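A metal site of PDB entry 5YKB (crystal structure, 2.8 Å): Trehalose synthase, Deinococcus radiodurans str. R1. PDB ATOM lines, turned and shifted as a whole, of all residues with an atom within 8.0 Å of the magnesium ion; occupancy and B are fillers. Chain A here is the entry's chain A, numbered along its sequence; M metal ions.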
ATOM      1  N   VAL A  21       0.409  -0.953 -19.721  1.00  0.00           N
ATOM      2  CA  VAL A  21      -0.657  -1.951 -19.587  1.00  0.00           C
ATOM      3  C   VAL A  21      -0.831  -2.769 -20.863  1.00  0.00           C
ATOM      4  O   VAL A  21      -1.098  -3.964 -20.808  1.00  0.00           O
ATOM      5  CB  VAL A  21      -2.005  -1.288 -19.199  1.00  0.00           C
ATOM      6  CG1 VAL A  21      -3.140  -2.299 -19.235  1.00  0.00           C
ATOM      7  CG2 VAL A  21      -1.906  -0.665 -17.804  1.00  0.00           C
ATOM      8  N   ARG A  22      -0.669  -2.136 -22.004  1.00  0.00           N
ATOM      9  CA  ARG A  22      -0.925  -2.782 -23.295  1.00  0.00           C
ATOM     10  C   ARG A  22       0.092  -3.840 -23.700  1.00  0.00           C
ATOM     11  O   ARG A  22      -0.134  -4.605 -24.640  1.00  0.00           O
ATOM     12  CB  ARG A  22      -1.016  -1.710 -24.384  1.00  0.00           C
ATOM     13  CG  ARG A  22      -1.882  -2.094 -25.568  1.00  0.00           C
ATOM     14  CD  ARG A  22      -2.007  -0.939 -26.545  1.00  0.00           C
ATOM     15  NE  ARG A  22      -2.233   0.342 -25.876  1.00  0.00           N
ATOM     16  CZ  ARG A  22      -3.349   1.067 -25.885  1.00  0.00           C
ATOM     17  NH1 ARG A  22      -4.435   0.647 -26.543  1.00  0.00           N
ATOM     18  NH2 ARG A  22      -3.385   2.211 -25.227  1.00  0.00           N
ATOM     19  N   GLN A  25       0.679  -7.755 -19.784  1.00  0.00           N
ATOM     20  CA  GLN A  25       0.001  -9.061 -19.809  1.00  0.00           C
ATOM     21  C   GLN A  25      -1.367  -9.002 -20.497  1.00  0.00           C
ATOM     22  O   GLN A  25      -2.250  -8.219 -20.113  1.00  0.00           O
ATOM     23  CB  GLN A  25      -0.194  -9.566 -18.384  1.00  0.00           C
ATOM     24  CG  GLN A  25      -0.782 -10.956 -18.286  1.00  0.00           C
ATOM     25  CD  GLN A  25       0.137 -12.008 -18.907  1.00  0.00           C
ATOM     26  OE1 GLN A  25       1.292 -12.126 -18.508  1.00  0.00           O
ATOM     27  NE2 GLN A  25      -0.361 -12.757 -19.878  1.00  0.00           N
ATOM     28  N   ASP A  26      -1.537  -9.869 -21.496  1.00  0.00           N
ATOM     29  CA  ASP A  26      -2.825 -10.031 -22.176  1.00  0.00           C
ATOM     30  C   ASP A  26      -3.648 -11.029 -21.380  1.00  0.00           C
ATOM     31  O   ASP A  26      -3.168 -12.079 -21.043  1.00  0.00           O
ATOM     32  CB  ASP A  26      -2.611 -10.543 -23.592  1.00  0.00           C
ATOM     33  CG  ASP A  26      -3.913 -10.734 -24.364  1.00  0.00           C
ATOM     34  OD1 ASP A  26      -4.940 -10.102 -23.972  1.00  0.00           O
ATOM     35  OD2 ASP A  26      -3.884 -11.485 -25.370  1.00  0.00           O
ATOM     36  N   GLY A  27      -4.890 -10.682 -21.117  1.00  0.00           N
ATOM     37  CA  GLY A  27      -5.760 -11.477 -20.255  1.00  0.00           C
ATOM     38  C   GLY A  27      -6.880 -12.201 -20.994  1.00  0.00           C
ATOM     39  O   GLY A  27      -7.584 -13.027 -20.402  1.00  0.00           O
ATOM     40  N   ASN A  28      -7.024 -11.886 -22.274  1.00  0.00           N
ATOM     41  CA  ASN A  28      -8.109 -12.442 -23.078  1.00  0.00           C
ATOM     42  C   ASN A  28      -7.746 -12.975 -24.471  1.00  0.00           C
ATOM     43  O   ASN A  28      -8.620 -13.273 -25.267  1.00  0.00           O
ATOM     44  CB  ASN A  28      -9.229 -11.411 -23.202  1.00  0.00           C
ATOM     45  CG  ASN A  28      -8.887 -10.287 -24.151  1.00  0.00           C
ATOM     46  OD1 ASN A  28      -7.723  -9.930 -24.358  1.00  0.00           O
ATOM     47  ND2 ASN A  28      -9.895  -9.701 -24.731  1.00  0.00           N
ATOM     48  N   GLY A  29      -6.464 -13.105 -24.764  1.00  0.00           N
ATOM     49  CA  GLY A  29      -6.065 -13.719 -26.012  1.00  0.00           C
ATOM     50  C   GLY A  29      -6.166 -12.875 -27.254  1.00  0.00           C
ATOM     51  O   GLY A  29      -5.914 -13.363 -28.333  1.00  0.00           O
ATOM     52  N   ASP A  30      -6.506 -11.591 -27.120  1.00  0.00           N
ATOM     53  CA  ASP A  30      -6.634 -10.673 -28.271  1.00  0.00           C
ATOM     54  C   ASP A  30      -5.298 -10.153 -28.781  1.00  0.00           C
ATOM     55  O   ASP A  30      -5.274  -9.373 -29.704  1.00  0.00           O
ATOM     56  CB  ASP A  30      -7.583  -9.503 -27.951  1.00  0.00           C
ATOM     57  CG  ASP A  30      -7.039  -8.540 -26.903  1.00  0.00           C
ATOM     58  OD1 ASP A  30      -5.954  -8.783 -26.320  1.00  0.00           O
ATOM     59  OD2 ASP A  30      -7.740  -7.539 -26.616  1.00  0.00           O
ATOM     60  N   GLY A  31      -4.210 -10.529 -28.136  1.00  0.00           N
ATOM     61  CA  GLY A  31      -2.882  -9.986 -28.444  1.00  0.00           C
ATOM     62  C   GLY A  31      -2.537  -8.620 -27.843  1.00  0.00           C
ATOM     63  O   GLY A  31      -1.455  -8.090 -28.115  1.00  0.00           O
ATOM     64  N   LYS A  32      -3.411  -8.062 -27.022  1.00  0.00           N
ATOM     65  CA  LYS A  32      -3.139  -6.767 -26.385  1.00  0.00           C
ATOM     66  C   LYS A  32      -3.240  -6.879 -24.886  1.00  0.00           C
ATOM     67  O   LYS A  32      -4.194  -7.452 -24.366  1.00  0.00           O
ATOM     68  CB  LYS A  32      -4.117  -5.678 -26.825  1.00  0.00           C
ATOM     69  CG  LYS A  32      -4.531  -5.713 -28.285  1.00  0.00           C
ATOM     70  CD  LYS A  32      -5.429  -4.536 -28.612  1.00  0.00           C
ATOM     71  CE  LYS A  32      -6.232  -4.800 -29.859  1.00  0.00           C
ATOM     72  NZ  LYS A  32      -6.527  -3.543 -30.585  1.00  0.00           N
ATOM     73  N   GLY A  33      -2.276  -6.274 -24.209  1.00  0.00           N
ATOM     74  CA  GLY A  33      -2.265  -6.198 -22.763  1.00  0.00           C
ATOM     75  C   GLY A  33      -3.465  -5.472 -22.213  1.00  0.00           C
ATOM     76  O   GLY A  33      -4.096  -4.693 -22.907  1.00  0.00           O
ATOM     77  N   ASP A  34      -3.789  -5.756 -20.960  1.00  0.00           N
ATOM     78  CA  ASP A  34      -5.008  -5.236 -20.312  1.00  0.00           C
ATOM     79  C   ASP A  34      -4.997  -5.375 -18.805  1.00  0.00           C
ATOM     80  O   ASP A  34      -4.170  -6.055 -18.226  1.00  0.00           O
ATOM     81  CB  ASP A  34      -6.267  -5.913 -20.897  1.00  0.00           C
ATOM     82  CG  ASP A  34      -6.236  -7.444 -20.820  1.00  0.00           C
ATOM     83  OD1 ASP A  34      -6.418  -7.988 -19.696  1.00  0.00           O
ATOM     84  OD2 ASP A  34      -6.095  -8.108 -21.881  1.00  0.00           O
ATOM     85  N   PHE A  35      -5.956  -4.711 -18.165  1.00  0.00           N
ATOM     86  CA  PHE A  35      -5.992  -4.632 -16.691  1.00  0.00           C
ATOM     87  C   PHE A  35      -6.154  -5.997 -16.004  1.00  0.00           C
ATOM     88  O   PHE A  35      -5.407  -6.295 -15.067  1.00  0.00           O
ATOM     89  CB  PHE A  35      -7.012  -3.598 -16.215  1.00  0.00           C
ATOM     90  CG  PHE A  35      -6.492  -2.189 -16.261  1.00  0.00           C
ATOM     91  CD1 PHE A  35      -5.657  -1.712 -15.243  1.00  0.00           C
ATOM     92  CD2 PHE A  35      -6.793  -1.355 -17.329  1.00  0.00           C
ATOM     93  CE1 PHE A  35      -5.160  -0.406 -15.296  1.00  0.00           C
ATOM     94  CE2 PHE A  35      -6.295  -0.059 -17.382  1.00  0.00           C
ATOM     95  CZ  PHE A  35      -5.481   0.415 -16.354  1.00  0.00           C
ATOM     96  N   PRO A  36      -7.113  -6.821 -16.464  1.00  0.00           N
ATOM     97  CA  PRO A  36      -7.226  -8.173 -15.953  1.00  0.00           C
ATOM     98  C   PRO A  36      -5.892  -8.940 -15.972  1.00  0.00           C
ATOM     99  O   PRO A  36      -5.487  -9.466 -14.961  1.00  0.00           O
ATOM    100  CB  PRO A  36      -8.258  -8.809 -16.879  1.00  0.00           C
ATOM    101  CG  PRO A  36      -9.149  -7.672 -17.193  1.00  0.00           C
ATOM    102  CD  PRO A  36      -8.219  -6.508 -17.386  1.00  0.00           C
ATOM    103  N   GLY A  37      -5.224  -8.929 -17.107  1.00  0.00           N
ATOM    104  CA  GLY A  37      -3.873  -9.469 -17.209  1.00  0.00           C
ATOM    105  C   GLY A  37      -2.883  -8.840 -16.228  1.00  0.00           C
ATOM    106  O   GLY A  37      -2.133  -9.522 -15.569  1.00  0.00           O
ATOM    107  N   PRO A  78     -10.978   1.166 -24.472  1.00  0.00           N
ATOM    108  CA  PRO A  78     -11.742  -0.065 -24.642  1.00  0.00           C
ATOM    109  C   PRO A  78     -10.926  -1.370 -24.728  1.00  0.00           C
ATOM    110  O   PRO A  78     -11.376  -2.422 -24.235  1.00  0.00           O
ATOM    111  CB  PRO A  78     -12.517   0.161 -25.955  1.00  0.00           C
ATOM    112  CG  PRO A  78     -11.757   1.209 -26.678  1.00  0.00           C
ATOM    113  CD  PRO A  78     -11.248   2.106 -25.577  1.00  0.00           C
ATOM    114  N   ASP A  79      -9.759  -1.322 -25.368  1.00  0.00           N
ATOM    115  CA  ASP A  79      -8.938  -2.523 -25.523  1.00  0.00           C
ATOM    116  C   ASP A  79      -7.974  -2.781 -24.348  1.00  0.00           C
ATOM    117  O   ASP A  79      -7.108  -3.646 -24.425  1.00  0.00           O
ATOM    118  CB  ASP A  79      -8.288  -2.607 -26.914  1.00  0.00           C
ATOM    119  CG  ASP A  79      -7.145  -1.647 -27.108  1.00  0.00           C
ATOM    120  OD1 ASP A  79      -6.459  -1.320 -26.110  1.00  0.00           O
ATOM    121  OD2 ASP A  79      -6.890  -1.245 -28.258  1.00  0.00           O
ATOM    122  N   LEU A  80      -8.174  -2.066 -23.250  1.00  0.00           N
ATOM    123  CA  LEU A  80      -7.485  -2.322 -21.970  1.00  0.00           C
ATOM    124  C   LEU A  80      -8.438  -2.872 -20.874  1.00  0.00           C
ATOM    125  O   LEU A  80      -7.986  -3.154 -19.744  1.00  0.00           O
ATOM    126  CB  LEU A  80      -6.841  -1.025 -21.464  1.00  0.00           C
ATOM    127  CG  LEU A  80      -5.379  -0.697 -21.785  1.00  0.00           C
ATOM    128  CD1 LEU A  80      -5.058  -0.759 -23.264  1.00  0.00           C
ATOM    129  CD2 LEU A  80      -5.051   0.689 -21.246  1.00  0.00           C
ATOM    130  N   GLY A  81      -9.727  -2.966 -21.189  1.00  0.00           N
ATOM    131  CA  GLY A  81     -10.764  -3.363 -20.201  1.00  0.00           C
ATOM    132  C   GLY A  81     -11.845  -2.320 -19.924  1.00  0.00           C
ATOM    133  O   GLY A  81     -12.129  -1.452 -20.744  1.00  0.00           O
ATOM    134  N   PHE A 417       3.069 -13.871 -22.693  1.00  0.00           N
ATOM    135  CA  PHE A 417       2.373 -12.587 -22.722  1.00  0.00           C
ATOM    136  C   PHE A 417       0.959 -12.719 -23.279  1.00  0.00           C
ATOM    137  O   PHE A 417       0.073 -11.915 -22.959  1.00  0.00           O
ATOM    138  CB  PHE A 417       3.151 -11.553 -23.547  1.00  0.00           C
ATOM    139  CG  PHE A 417       2.310 -10.414 -24.038  1.00  0.00           C
ATOM    140  CD1 PHE A 417       1.951  -9.378 -23.200  1.00  0.00           C
ATOM    141  CD2 PHE A 417       1.871 -10.387 -25.345  1.00  0.00           C
ATOM    142  CE1 PHE A 417       1.176  -8.322 -23.651  1.00  0.00           C
ATOM    143  CE2 PHE A 417       1.095  -9.341 -25.824  1.00  0.00           C
ATOM    144  CZ  PHE A 417       0.751  -8.303 -24.974  1.00  0.00           C
ATOM    145  N   SER A 418       0.755 -13.727 -24.119  1.00  0.00           N
ATOM    146  CA  SER A 418      -0.558 -13.987 -24.691  1.00  0.00           C
ATOM    147  C   SER A 418      -0.576 -15.382 -25.297  1.00  0.00           C
ATOM    148  O   SER A 418       0.446 -15.895 -25.665  1.00  0.00           O
ATOM    149  CB  SER A 418      -0.883 -12.934 -25.774  1.00  0.00           C
ATOM    150  OG  SER A 418      -2.090 -13.217 -26.458  1.00  0.00           O
HETATM  151 MG    MG M   1      -6.222  -8.197 -24.005  1.00  0.00          MG
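The backbone NH (N) of Gly 27 lies within hydrogen-bond range of the side-chain carboxylate (OD1) of Asp 34, 3.4 Å away. The backbone NH (N) of Asp 34 is in hydrogen-bond range of the backbone carbonyl oxygen (O) of Gln 25 (3.0 Å). The backbone NH (N) of Gly 37 lies within hydrogen-bond range of the side-chain carboxylate (OD1) of Asp 34, 3.0 Å away. The backbone carbonyl oxygen (O) of Val 21 is in hydrogen-bond range of the backbone NH (N) of Asp 34, at 3.2 Å. OD2 of Asp 79 is in salt-bridge range of NZ of Lys 32. N of Gly 29 is in hydrogen-bond range of OD2 of Asp 26 (3.1 Å). The backbone NH of Gly 31 sits at hydrogen-bond distance from the side-chain carboxylate of Asp 26, at 2.9 Å. N of Asp 26 is in hydrogen-bond range of O of Phe 417, 3.0 Å away.
The nearest printed residue that does not touch the magnesium ion is Gly 27 (4.04 Å).
The magnesium ion is bound by OD2 of Asp 34, 2.1 Å away. The magnesium ion is bound by O of Lys 32 (2.2 Å). The magnesium ion is bound by OD1 of Asp 26 (2.3 Å). OD1 of Asn 28 is bound to the magnesium ion, 2.3 Å away. The side-chain carboxylate (OD1) of Asp 30 is bound to the magnesium ion, 2.4 Å away.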
